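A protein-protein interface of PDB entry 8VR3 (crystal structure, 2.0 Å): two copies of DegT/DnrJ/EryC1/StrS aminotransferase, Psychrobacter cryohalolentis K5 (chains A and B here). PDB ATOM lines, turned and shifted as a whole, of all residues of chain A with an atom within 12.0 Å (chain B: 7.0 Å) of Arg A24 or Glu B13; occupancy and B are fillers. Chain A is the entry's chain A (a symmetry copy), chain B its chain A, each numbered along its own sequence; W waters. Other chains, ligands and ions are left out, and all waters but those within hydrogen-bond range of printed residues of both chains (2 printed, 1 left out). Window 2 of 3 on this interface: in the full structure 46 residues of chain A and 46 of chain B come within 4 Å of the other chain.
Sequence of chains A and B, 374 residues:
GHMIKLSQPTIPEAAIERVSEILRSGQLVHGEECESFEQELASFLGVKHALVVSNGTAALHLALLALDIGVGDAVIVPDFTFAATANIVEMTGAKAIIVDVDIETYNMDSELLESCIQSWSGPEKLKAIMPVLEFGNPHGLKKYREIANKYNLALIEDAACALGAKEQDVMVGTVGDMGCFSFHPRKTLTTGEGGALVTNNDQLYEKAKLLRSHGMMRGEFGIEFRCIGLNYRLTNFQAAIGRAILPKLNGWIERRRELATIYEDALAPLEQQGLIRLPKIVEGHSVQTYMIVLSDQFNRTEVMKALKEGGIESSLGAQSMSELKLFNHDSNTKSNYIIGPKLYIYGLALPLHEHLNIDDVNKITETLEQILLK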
ATOM      1  N   GLU A  13     -16.275 -31.635  -1.430  1.00  0.00           N
ATOM      2  CA  GLU A  13     -17.112 -31.468  -2.611  1.00  0.00           C
ATOM      3  C   GLU A  13     -18.084 -30.309  -2.434  1.00  0.00           C
ATOM      4  O   GLU A  13     -18.336 -29.595  -3.391  1.00  0.00           O
ATOM      5  CB  GLU A  13     -17.905 -32.736  -2.916  1.00  0.00           C
ATOM      6  CG  GLU A  13     -17.065 -33.823  -3.549  1.00  0.00           C
ATOM      7  CD  GLU A  13     -16.447 -33.434  -4.879  1.00  0.00           C
ATOM      8  OE1 GLU A  13     -17.115 -32.728  -5.660  1.00  0.00           O
ATOM      9  OE2 GLU A  13     -15.311 -33.856  -5.132  1.00  0.00           O
ATOM     10  N   ALA A  14     -18.594 -30.098  -1.217  1.00  0.00           N
ATOM     11  CA  ALA A  14     -19.449 -28.948  -0.959  1.00  0.00           C
ATOM     12  C   ALA A  14     -18.731 -27.661  -1.380  1.00  0.00           C
ATOM     13  O   ALA A  14     -19.294 -26.843  -2.115  1.00  0.00           O
ATOM     14  CB  ALA A  14     -19.855 -28.899   0.501  1.00  0.00           C
ATOM     15  N   ALA A  15     -17.496 -27.498  -0.879  1.00  0.00           N
ATOM     16  CA  ALA A  15     -16.651 -26.367  -1.226  1.00  0.00           C
ATOM     17  C   ALA A  15     -16.486 -26.247  -2.746  1.00  0.00           C
ATOM     18  O   ALA A  15     -16.580 -25.165  -3.314  1.00  0.00           O
ATOM     19  CB  ALA A  15     -15.321 -26.507  -0.542  1.00  0.00           C
ATOM     20  N   ILE A  16     -16.222 -27.363  -3.416  1.00  0.00           N
ATOM     21  CA  ILE A  16     -16.055 -27.312  -4.858  1.00  0.00           C
ATOM     22  C   ILE A  16     -17.309 -26.743  -5.538  1.00  0.00           C
ATOM     23  O   ILE A  16     -17.197 -25.942  -6.465  1.00  0.00           O
ATOM     24  CB  ILE A  16     -15.655 -28.698  -5.379  1.00  0.00           C
ATOM     25  CG1 ILE A  16     -14.263 -29.072  -4.852  1.00  0.00           C
ATOM     26  CG2 ILE A  16     -15.747 -28.759  -6.895  1.00  0.00           C
ATOM     27  CD1 ILE A  16     -13.756 -30.413  -5.309  1.00  0.00           C
ATOM     28  N   GLU A  17     -18.502 -27.147  -5.081  1.00  0.00           N
ATOM     29  CA  GLU A  17     -19.750 -26.699  -5.689  1.00  0.00           C
ATOM     30  C   GLU A  17     -19.982 -25.225  -5.378  1.00  0.00           C
ATOM     31  O   GLU A  17     -20.399 -24.481  -6.244  1.00  0.00           O
ATOM     32  CB  GLU A  17     -20.946 -27.536  -5.229  1.00  0.00           C
ATOM     33  CG  GLU A  17     -20.996 -28.909  -5.890  1.00  0.00           C
ATOM     34  CD  GLU A  17     -21.854 -29.933  -5.153  1.00  0.00           C
ATOM     35  OE1 GLU A  17     -23.061 -29.645  -4.928  1.00  0.00           O
ATOM     36  OE2 GLU A  17     -21.322 -31.018  -4.795  1.00  0.00           O
ATOM     37  N   ARG A  18     -19.649 -24.801  -4.159  1.00  0.00           N
ATOM     38  CA  ARG A  18     -19.778 -23.413  -3.771  1.00  0.00           C
ATOM     39  C   ARG A  18     -18.833 -22.509  -4.569  1.00  0.00           C
ATOM     40  O   ARG A  18     -19.244 -21.431  -5.005  1.00  0.00           O
ATOM     41  CB  ARG A  18     -19.548 -23.335  -2.268  1.00  0.00           C
ATOM     42  CG  ARG A  18     -19.810 -21.954  -1.715  1.00  0.00           C
ATOM     43  CD  ARG A  18     -21.265 -21.560  -1.820  1.00  0.00           C
ATOM     44  NE  ARG A  18     -21.315 -20.173  -1.423  1.00  0.00           N
ATOM     45  CZ  ARG A  18     -21.775 -19.196  -2.180  1.00  0.00           C
ATOM     46  NH1 ARG A  18     -22.511 -19.484  -3.231  1.00  0.00           N
ATOM     47  NH2 ARG A  18     -21.542 -17.937  -1.851  1.00  0.00           N
ATOM     48  N   VAL A  19     -17.589 -22.965  -4.801  1.00  0.00           N
ATOM     49  CA  VAL A  19     -16.661 -22.221  -5.646  1.00  0.00           C
ATOM     50  C   VAL A  19     -17.273 -22.051  -7.047  1.00  0.00           C
ATOM     51  O   VAL A  19     -17.193 -20.971  -7.660  1.00  0.00           O
ATOM     52  CB  VAL A  19     -15.259 -22.872  -5.711  1.00  0.00           C
ATOM     53  CG1 VAL A  19     -14.426 -22.270  -6.833  1.00  0.00           C
ATOM     54  CG2 VAL A  19     -14.493 -22.779  -4.390  1.00  0.00           C
ATOM     55  N   SER A  20     -17.912 -23.115  -7.547  1.00  0.00           N
ATOM     56  CA  SER A  20     -18.518 -23.060  -8.871  1.00  0.00           C
ATOM     57  C   SER A  20     -19.660 -22.046  -8.885  1.00  0.00           C
ATOM     58  O   SER A  20     -19.751 -21.271  -9.832  1.00  0.00           O
ATOM     59  CB  SER A  20     -18.997 -24.413  -9.342  1.00  0.00           C
ATOM     60  OG  SER A  20     -17.898 -25.278  -9.525  1.00  0.00           O
ATOM     61  N   GLU A  21     -20.485 -22.019  -7.824  1.00  0.00           N
ATOM     62  CA  GLU A  21     -21.573 -21.050  -7.739  1.00  0.00           C
ATOM     63  C   GLU A  21     -21.002 -19.626  -7.735  1.00  0.00           C
ATOM     64  O   GLU A  21     -21.526 -18.745  -8.413  1.00  0.00           O
ATOM     65  CB  GLU A  21     -22.442 -21.166  -6.471  1.00  0.00           C
ATOM     66  CG  GLU A  21     -23.260 -22.452  -6.271  1.00  0.00           C
ATOM     67  CD  GLU A  21     -23.754 -22.660  -4.828  1.00  0.00           C
ATOM     68  OE1 GLU A  21     -24.257 -21.677  -4.211  1.00  0.00           O
ATOM     69  OE2 GLU A  21     -23.612 -23.794  -4.287  1.00  0.00           O
ATOM     70  N   ILE A  22     -19.963 -19.374  -6.924  1.00  0.00           N
ATOM     71  CA  ILE A  22     -19.389 -18.036  -6.831  1.00  0.00           C
ATOM     72  C   ILE A  22     -18.842 -17.581  -8.190  1.00  0.00           C
ATOM     73  O   ILE A  22     -19.095 -16.470  -8.631  1.00  0.00           O
ATOM     74  CB  ILE A  22     -18.324 -17.982  -5.721  1.00  0.00           C
ATOM     75  CG1 ILE A  22     -18.963 -18.166  -4.349  1.00  0.00           C
ATOM     76  CG2 ILE A  22     -17.509 -16.696  -5.773  1.00  0.00           C
ATOM     77  CD1 ILE A  22     -17.980 -18.565  -3.278  1.00  0.00           C
ATOM     78  N   LEU A  23     -18.060 -18.422  -8.857  1.00  0.00           N
ATOM     79  CA  LEU A  23     -17.481 -18.074 -10.142  1.00  0.00           C
ATOM     80  C   LEU A  23     -18.578 -17.760 -11.167  1.00  0.00           C
ATOM     81  O   LEU A  23     -18.432 -16.822 -11.958  1.00  0.00           O
ATOM     82  CB  LEU A  23     -16.560 -19.226 -10.599  1.00  0.00           C
ATOM     83  CG  LEU A  23     -15.257 -19.399  -9.803  1.00  0.00           C
ATOM     84  CD1 LEU A  23     -14.428 -20.588 -10.300  1.00  0.00           C
ATOM     85  CD2 LEU A  23     -14.416 -18.146  -9.891  1.00  0.00           C
ATOM     86  N   ARG A  24     -19.673 -18.529 -11.147  1.00  0.00           N
ATOM     87  CA  ARG A  24     -20.737 -18.409 -12.131  1.00  0.00           C
ATOM     88  C   ARG A  24     -21.557 -17.141 -11.909  1.00  0.00           C
ATOM     89  O   ARG A  24     -21.938 -16.486 -12.855  1.00  0.00           O
ATOM     90  CB  ARG A  24     -21.630 -19.656 -12.077  1.00  0.00           C
ATOM     91  CG  ARG A  24     -22.638 -19.740 -13.213  1.00  0.00           C
ATOM     92  CD  ARG A  24     -23.227 -21.128 -13.373  1.00  0.00           C
ATOM     93  NE  ARG A  24     -22.201 -22.105 -13.713  1.00  0.00           N
ATOM     94  CZ  ARG A  24     -21.905 -23.172 -12.980  1.00  0.00           C
ATOM     95  NH1 ARG A  24     -22.466 -23.334 -11.800  1.00  0.00           N
ATOM     96  NH2 ARG A  24     -21.056 -24.079 -13.421  1.00  0.00           N
ATOM     97  N   SER A  25     -21.804 -16.793 -10.656  1.00  0.00           N
ATOM     98  CA  SER A  25     -22.570 -15.620 -10.286  1.00  0.00           C
ATOM     99  C   SER A  25     -21.759 -14.334 -10.405  1.00  0.00           C
ATOM    100  O   SER A  25     -22.349 -13.260 -10.303  1.00  0.00           O
ATOM    101  CB  SER A  25     -22.954 -15.706  -8.869  1.00  0.00           C
ATOM    102  OG  SER A  25     -21.835 -15.283  -8.102  1.00  0.00           O
ATOM    103  N   GLY A  26     -20.412 -14.447 -10.421  1.00  0.00           N
ATOM    104  CA  GLY A  26     -19.505 -13.311 -10.551  1.00  0.00           C
ATOM    105  C   GLY A  26     -19.339 -12.450  -9.288  1.00  0.00           C
ATOM    106  O   GLY A  26     -18.977 -11.280  -9.417  1.00  0.00           O
ATOM    107  N   GLN A  27     -19.517 -13.025  -8.083  1.00  0.00           N
ATOM    108  CA  GLN A  27     -19.276 -12.339  -6.808  1.00  0.00           C
ATOM    109  C   GLN A  27     -17.899 -12.650  -6.193  1.00  0.00           C
ATOM    110  O   GLN A  27     -17.811 -13.387  -5.207  1.00  0.00           O
ATOM    111  CB  GLN A  27     -20.351 -12.781  -5.819  1.00  0.00           C
ATOM    112  CG  GLN A  27     -21.755 -12.304  -6.178  1.00  0.00           C
ATOM    113  CD  GLN A  27     -22.832 -13.057  -5.424  1.00  0.00           C
ATOM    114  OE1 GLN A  27     -22.603 -14.143  -4.888  1.00  0.00           O
ATOM    115  NE2 GLN A  27     -24.034 -12.497  -5.397  1.00  0.00           N
ATOM    116  N   LEU A  28     -16.826 -12.015  -6.691  1.00  0.00           N
ATOM    117  CA  LEU A  28     -15.480 -12.578  -6.605  1.00  0.00           C
ATOM    118  C   LEU A  28     -14.601 -11.999  -5.483  1.00  0.00           C
ATOM    119  O   LEU A  28     -13.840 -12.738  -4.837  1.00  0.00           O
ATOM    120  CB  LEU A  28     -14.809 -12.352  -7.958  1.00  0.00           C
ATOM    121  CG  LEU A  28     -15.511 -13.019  -9.133  1.00  0.00           C
ATOM    122  CD1 LEU A  28     -14.665 -12.917 -10.396  1.00  0.00           C
ATOM    123  CD2 LEU A  28     -15.819 -14.475  -8.803  1.00  0.00           C
ATOM    124  N   VAL A  29     -14.599 -10.667  -5.343  1.00  0.00           N
ATOM    125  CA  VAL A  29     -13.713  -9.968  -4.412  1.00  0.00           C
ATOM    126  C   VAL A  29     -14.139 -10.311  -2.981  1.00  0.00           C
ATOM    127  O   VAL A  29     -15.310 -10.621  -2.762  1.00  0.00           O
ATOM    128  CB  VAL A  29     -13.752  -8.438  -4.658  1.00  0.00           C
ATOM    129  CG1 VAL A  29     -15.088  -7.796  -4.246  1.00  0.00           C
ATOM    130  CG2 VAL A  29     -12.571  -7.717  -4.013  1.00  0.00           C
ATOM    131  N   GLU A  33     -18.279 -13.786   2.152  1.00  0.00           N
ATOM    132  CA  GLU A  33     -17.630 -15.066   2.348  1.00  0.00           C
ATOM    133  C   GLU A  33     -16.391 -14.902   3.242  1.00  0.00           C
ATOM    134  O   GLU A  33     -16.211 -15.659   4.204  1.00  0.00           O
ATOM    135  CB  GLU A  33     -17.350 -15.636   0.965  1.00  0.00           C
ATOM    136  CG  GLU A  33     -17.371 -17.121   0.901  1.00  0.00           C
ATOM    137  CD  GLU A  33     -18.695 -17.818   1.105  1.00  0.00           C
ATOM    138  OE1 GLU A  33     -19.702 -17.409   0.514  1.00  0.00           O
ATOM    139  OE2 GLU A  33     -18.678 -18.840   1.799  1.00  0.00           O
ATOM    140  N   THR A 235      -9.553 -13.913  -2.088  1.00  0.00           N
ATOM    141  CA  THR A 235     -10.791 -13.995  -2.846  1.00  0.00           C
ATOM    142  C   THR A 235     -11.900 -14.624  -1.997  1.00  0.00           C
ATOM    143  O   THR A 235     -11.696 -15.465  -1.132  1.00  0.00           O
ATOM    144  CB  THR A 235     -10.697 -14.766  -4.174  1.00  0.00           C
ATOM    145  OG1 THR A 235     -10.539 -16.178  -3.955  1.00  0.00           O
ATOM    146  CG2 THR A 235      -9.578 -14.268  -5.055  1.00  0.00           C
ATOM    147  N   ASN A 236     -13.105 -14.210  -2.324  1.00  0.00           N
ATOM    148  CA  ASN A 236     -14.335 -14.785  -1.829  1.00  0.00           C
ATOM    149  C   ASN A 236     -14.389 -16.302  -2.006  1.00  0.00           C
ATOM    150  O   ASN A 236     -14.872 -17.003  -1.113  1.00  0.00           O
ATOM    151  CB  ASN A 236     -15.492 -14.115  -2.568  1.00  0.00           C
ATOM    152  CG  ASN A 236     -16.673 -13.861  -1.676  1.00  0.00           C
ATOM    153  OD1 ASN A 236     -16.492 -13.344  -0.567  1.00  0.00           O
ATOM    154  ND2 ASN A 236     -17.861 -14.217  -2.159  1.00  0.00           N
ATOM    155  N   PHE A 237     -13.982 -16.811  -3.176  1.00  0.00           N
ATOM    156  CA  PHE A 237     -14.084 -18.237  -3.429  1.00  0.00           C
ATOM    157  C   PHE A 237     -13.007 -19.028  -2.686  1.00  0.00           C
ATOM    158  O   PHE A 237     -13.258 -20.164  -2.313  1.00  0.00           O
ATOM    159  CB  PHE A 237     -14.175 -18.541  -4.927  1.00  0.00           C
ATOM    160  CG  PHE A 237     -13.062 -18.031  -5.797  1.00  0.00           C
ATOM    161  CD1 PHE A 237     -13.175 -16.800  -6.412  1.00  0.00           C
ATOM    162  CD2 PHE A 237     -11.937 -18.798  -6.033  1.00  0.00           C
ATOM    163  CE1 PHE A 237     -12.178 -16.315  -7.229  1.00  0.00           C
ATOM    164  CE2 PHE A 237     -10.937 -18.313  -6.862  1.00  0.00           C
ATOM    165  CZ  PHE A 237     -11.066 -17.069  -7.460  1.00  0.00           C
ATOM    166  N   GLN A 238     -11.837 -18.440  -2.428  1.00  0.00           N
ATOM    167  CA  GLN A 238     -10.853 -19.044  -1.532  1.00  0.00           C
ATOM    168  C   GLN A 238     -11.382 -19.085  -0.103  1.00  0.00           C
ATOM    169  O   GLN A 238     -11.219 -20.088   0.583  1.00  0.00           O
ATOM    170  CB  GLN A 238      -9.509 -18.315  -1.582  1.00  0.00           C
ATOM    171  CG  GLN A 238      -8.765 -18.572  -2.871  1.00  0.00           C
ATOM    172  CD  GLN A 238      -7.665 -17.556  -3.043  1.00  0.00           C
ATOM    173  OE1 GLN A 238      -7.907 -16.405  -3.422  1.00  0.00           O
ATOM    174  NE2 GLN A 238      -6.461 -17.979  -2.694  1.00  0.00           N
ATOM    175  N   ALA A 240     -14.444 -19.431   0.751  1.00  0.00           N
ATOM    176  CA  ALA A 240     -15.478 -20.453   0.830  1.00  0.00           C
ATOM    177  C   ALA A 240     -14.867 -21.826   1.090  1.00  0.00           C
ATOM    178  O   ALA A 240     -15.443 -22.654   1.791  1.00  0.00           O
ATOM    179  CB  ALA A 240     -16.237 -20.467  -0.484  1.00  0.00           C
ATOM    180  N   GLN B   8     -19.934  -7.231 -14.266  1.00  0.00           N
ATOM    181  CA  GLN B   8     -20.487  -8.572 -14.214  1.00  0.00           C
ATOM    182  C   GLN B   8     -19.371  -9.509 -14.674  1.00  0.00           C
ATOM    183  O   GLN B   8     -19.263  -9.821 -15.864  1.00  0.00           O
ATOM    184  CB  GLN B   8     -21.733  -8.665 -15.094  1.00  0.00           C
ATOM    185  CG  GLN B   8     -22.477  -9.991 -14.998  1.00  0.00           C
ATOM    186  CD  GLN B   8     -23.656 -10.099 -15.949  1.00  0.00           C
ATOM    187  OE1 GLN B   8     -23.733 -11.005 -16.784  1.00  0.00           O
ATOM    188  NE2 GLN B   8     -24.609  -9.183 -15.830  1.00  0.00           N
ATOM    189  N   PRO B   9     -18.465  -9.914 -13.751  1.00  0.00           N
ATOM    190  CA  PRO B   9     -17.352 -10.790 -14.093  1.00  0.00           C
ATOM    191  C   PRO B   9     -17.787 -12.064 -14.813  1.00  0.00           C
ATOM    192  O   PRO B   9     -18.747 -12.744 -14.417  1.00  0.00           O
ATOM    193  CB  PRO B   9     -16.736 -11.120 -12.726  1.00  0.00           C
ATOM    194  CG  PRO B   9     -17.045  -9.896 -11.897  1.00  0.00           C
ATOM    195  CD  PRO B   9     -18.451  -9.531 -12.328  1.00  0.00           C
ATOM    196  N   THR B  10     -17.008 -12.372 -15.852  1.00  0.00           N
ATOM    197  CA  THR B  10     -17.322 -13.419 -16.798  1.00  0.00           C
ATOM    198  C   THR B  10     -16.251 -14.506 -16.681  1.00  0.00           C
ATOM    199  O   THR B  10     -15.162 -14.346 -17.199  1.00  0.00           O
ATOM    200  CB  THR B  10     -17.452 -12.823 -18.218  1.00  0.00           C
ATOM    201  OG1 THR B  10     -18.494 -11.848 -18.221  1.00  0.00           O
ATOM    202  CG2 THR B  10     -17.743 -13.869 -19.273  1.00  0.00           C
ATOM    203  N   ILE B  11     -16.604 -15.611 -16.010  1.00  0.00           N
ATOM    204  CA  ILE B  11     -15.777 -16.788 -15.891  1.00  0.00           C
ATOM    205  C   ILE B  11     -16.340 -17.841 -16.839  1.00  0.00           C
ATOM    206  O   ILE B  11     -17.410 -18.392 -16.589  1.00  0.00           O
ATOM    207  CB  ILE B  11     -15.759 -17.333 -14.439  1.00  0.00           C
ATOM    208  CG1 ILE B  11     -15.542 -16.243 -13.376  1.00  0.00           C
ATOM    209  CG2 ILE B  11     -14.756 -18.485 -14.320  1.00  0.00           C
ATOM    210  CD1 ILE B  11     -14.447 -15.252 -13.703  1.00  0.00           C
ATOM    211  N   PRO B  12     -15.638 -18.184 -17.930  1.00  0.00           N
ATOM    212  CA  PRO B  12     -16.145 -19.187 -18.867  1.00  0.00           C
ATOM    213  C   PRO B  12     -16.377 -20.530 -18.171  1.00  0.00           C
ATOM    214  O   PRO B  12     -15.630 -20.895 -17.268  1.00  0.00           O
ATOM    215  CB  PRO B  12     -15.026 -19.317 -19.903  1.00  0.00           C
ATOM    216  CG  PRO B  12     -14.252 -18.022 -19.792  1.00  0.00           C
ATOM    217  CD  PRO B  12     -14.359 -17.600 -18.344  1.00  0.00           C
ATOM    218  N   GLU B  13     -17.437 -21.236 -18.577  1.00  0.00           N
ATOM    219  CA  GLU B  13     -17.796 -22.523 -17.993  1.00  0.00           C
ATOM    220  C   GLU B  13     -16.635 -23.505 -18.076  1.00  0.00           C
ATOM    221  O   GLU B  13     -16.441 -24.273 -17.148  1.00  0.00           O
ATOM    222  CB  GLU B  13     -19.009 -23.132 -18.690  1.00  0.00           C
ATOM    223  CG  GLU B  13     -20.313 -22.479 -18.290  1.00  0.00           C
ATOM    224  CD  GLU B  13     -20.633 -22.589 -16.811  1.00  0.00           C
ATOM    225  OE1 GLU B  13     -20.339 -23.645 -16.217  1.00  0.00           O
ATOM    226  OE2 GLU B  13     -21.191 -21.626 -16.268  1.00  0.00           O
ATOM    227  N   ALA B  14     -15.846 -23.454 -19.153  1.00  0.00           N
ATOM    228  CA  ALA B  14     -14.662 -24.297 -19.247  1.00  0.00           C
ATOM    229  C   ALA B  14     -13.769 -24.076 -18.021  1.00  0.00           C
ATOM    230  O   ALA B  14     -13.361 -25.039 -17.363  1.00  0.00           O
ATOM    231  CB  ALA B  14     -13.908 -24.021 -20.533  1.00  0.00           C
ATOM    232  N   ALA B  15     -13.463 -22.797 -17.751  1.00  0.00           N
ATOM    233  CA  ALA B  15     -12.679 -22.405 -16.591  1.00  0.00           C
ATOM    234  C   ALA B  15     -13.299 -22.949 -15.298  1.00  0.00           C
ATOM    235  O   ALA B  15     -12.608 -23.473 -14.431  1.00  0.00           O
ATOM    236  CB  ALA B  15     -12.560 -20.907 -16.550  1.00  0.00           C
ATOM    237  N   ILE B  16     -14.612 -22.815 -15.153  1.00  0.00           N
ATOM    238  CA  ILE B  16     -15.255 -23.312 -13.948  1.00  0.00           C
ATOM    239  C   ILE B  16     -15.000 -24.815 -13.768  1.00  0.00           C
ATOM    240  O   ILE B  16     -14.737 -25.266 -12.653  1.00  0.00           O
ATOM    241  CB  ILE B  16     -16.745 -22.945 -13.971  1.00  0.00           C
ATOM    242  CG1 ILE B  16     -16.907 -21.421 -13.885  1.00  0.00           C
ATOM    243  CG2 ILE B  16     -17.505 -23.682 -12.882  1.00  0.00           C
ATOM    244  CD1 ILE B  16     -18.333 -20.940 -13.887  1.00  0.00           C
ATOM    245  N   GLU B  17     -15.070 -25.594 -14.856  1.00  0.00           N
ATOM    246  CA  GLU B  17     -14.888 -27.039 -14.780  1.00  0.00           C
ATOM    247  C   GLU B  17     -13.430 -27.366 -14.478  1.00  0.00           C
ATOM    248  O   GLU B  17     -13.157 -28.245 -13.685  1.00  0.00           O
ATOM    249  CB  GLU B  17     -15.338 -27.742 -16.064  1.00  0.00           C
ATOM    250  CG  GLU B  17     -16.855 -27.836 -16.185  1.00  0.00           C
ATOM    251  CD  GLU B  17     -17.359 -28.086 -17.603  1.00  0.00           C
ATOM    252  OE1 GLU B  17     -16.928 -29.101 -18.216  1.00  0.00           O
ATOM    253  OE2 GLU B  17     -18.178 -27.270 -18.104  1.00  0.00           O
ATOM    254  N   ARG B  18     -12.503 -26.611 -15.068  1.00  0.00           N
ATOM    255  CA  ARG B  18     -11.091 -26.798 -14.814  1.00  0.00           C
ATOM    256  C   ARG B  18     -10.726 -26.476 -13.362  1.00  0.00           C
ATOM    257  O   ARG B  18      -9.957 -27.220 -12.747  1.00  0.00           O
ATOM    258  CB  ARG B  18     -10.329 -25.947 -15.822  1.00  0.00           C
ATOM    259  CG  ARG B  18      -8.837 -26.178 -15.761  1.00  0.00           C
ATOM    260  CD  ARG B  18      -8.454 -27.575 -16.191  1.00  0.00           C
ATOM    261  NE  ARG B  18      -7.043 -27.688 -15.908  1.00  0.00           N
ATOM    262  CZ  ARG B  18      -6.512 -28.598 -15.115  1.00  0.00           C
ATOM    263  NH1 ARG B  18      -7.216 -29.658 -14.784  1.00  0.00           N
ATOM    264  NH2 ARG B  18      -5.262 -28.470 -14.703  1.00  0.00           N
ATOM    265  N   VAL B  19     -11.311 -25.403 -12.800  1.00  0.00           N
ATOM    266  CA  VAL B  19     -11.108 -25.088 -11.390  1.00  0.00           C
ATOM    267  C   VAL B  19     -11.580 -26.273 -10.531  1.00  0.00           C
ATOM    268  O   VAL B  19     -10.922 -26.663  -9.549  1.00  0.00           O
ATOM    269  CB  VAL B  19     -11.794 -23.768 -10.967  1.00  0.00           C
ATOM    270  CG1 VAL B  19     -11.840 -23.633  -9.452  1.00  0.00           C
ATOM    271  CG2 VAL B  19     -11.136 -22.529 -11.577  1.00  0.00           C
ATOM    272  N   LYS B 248     -10.098 -15.159 -25.411  1.00  0.00           N
ATOM    273  CA  LYS B 248     -11.304 -14.413 -25.729  1.00  0.00           C
ATOM    274  C   LYS B 248     -11.156 -12.897 -25.588  1.00  0.00           C
ATOM    275  O   LYS B 248     -12.074 -12.168 -25.975  1.00  0.00           O
ATOM    276  CB  LYS B 248     -12.439 -14.825 -24.791  1.00  0.00           C
ATOM    277  CG  LYS B 248     -12.645 -16.327 -24.636  1.00  0.00           C
ATOM    278  CD  LYS B 248     -13.735 -16.654 -23.659  1.00  0.00           C
ATOM    279  CE  LYS B 248     -13.888 -18.135 -23.442  1.00  0.00           C
ATOM    280  NZ  LYS B 248     -14.571 -18.721 -24.613  1.00  0.00           N
HETATM  281  O   HOH W   1     -15.448 -24.066 -10.165  1.00  0.00           O
HETATM  282  O   HOH W   2     -21.788 -13.772 -14.616  1.00  0.00           O
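The side-chain carboxylate of Glu B13 lies within salt-bridge range of the guanidinium group of Arg A24 (2.8 Å).
The backbone carbonyl oxygen of Ile A16 is in hydrogen-bond range of the side-chain hydroxyl of Ser A20, 3.2 Å away.
O of Leu A28 is in hydrogen-bond range of N of Asn A236 (3.0 Å).
Among the printed residues, merely in contact across the chains: Leu A23 with Ile B11 (3.3 Å), Gly A26 with Pro B9 (3.4 Å), Leu A28 with Pro B9 (3.6 Å), Arg A24 with Ile B16 (3.6 Å), Ser A20 with Ile B16 (3.7 Å), Val A19 with Val B19 (3.9 Å) and Leu A23 with Ile B16 (3.97 Å).
Ile B11 touches just one residue of chain A: Leu A23 (3.3 Å).
Pro B12 touches none of the printed residues of chain A.
No residue of chain A comes within 4 Å of Ala B14.
No residue of chain A comes within 4 Å of Ala B15.
Ile B16 touches three residues of chain A.
Of the printed residues of chain B, Leu A23 touches Ile B11 and Ile B16.
Of the printed residues of chain B, Leu A28 touches Pro B9.
Of the printed residues of chain B, Val A19 touches Val B19 (3.9 Å).
Printed residues of chain A within 4 Å of Pro B9: Gly A26 (3.4 Å) and Leu A28 (3.6 Å).
Glu A13 touches none of the printed residues of chain B.
The nearest residue of chain A that does not touch Glu B13 is Ser A20 (6.6 Å).
Printed residues of chain B that touch a printed residue of chain A: Pro B9, Ile B11, Glu B13, Ile B16 and Val B19.
Among the printed residues, 8 pairs touch across the chains.
Among the printed residues, Asp or Glu carboxylates within 4 Å of a Lys or Arg side-chain nitrogen of the other chain: Arg A24 with Glu B13 (2.8 Å).
Val B19 touches its own counterpart, Val A19.
Water W1 lies within hydrogen-bond range of the side-chain hydroxyl of Ser A20 and the backbone carbonyl oxygen of Ile B16.
Water W2 lies within hydrogen-bond range of the backbone carbonyl oxygen (O) of Pro B9 and the backbone carbonyl oxygen (O) of Arg A24.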
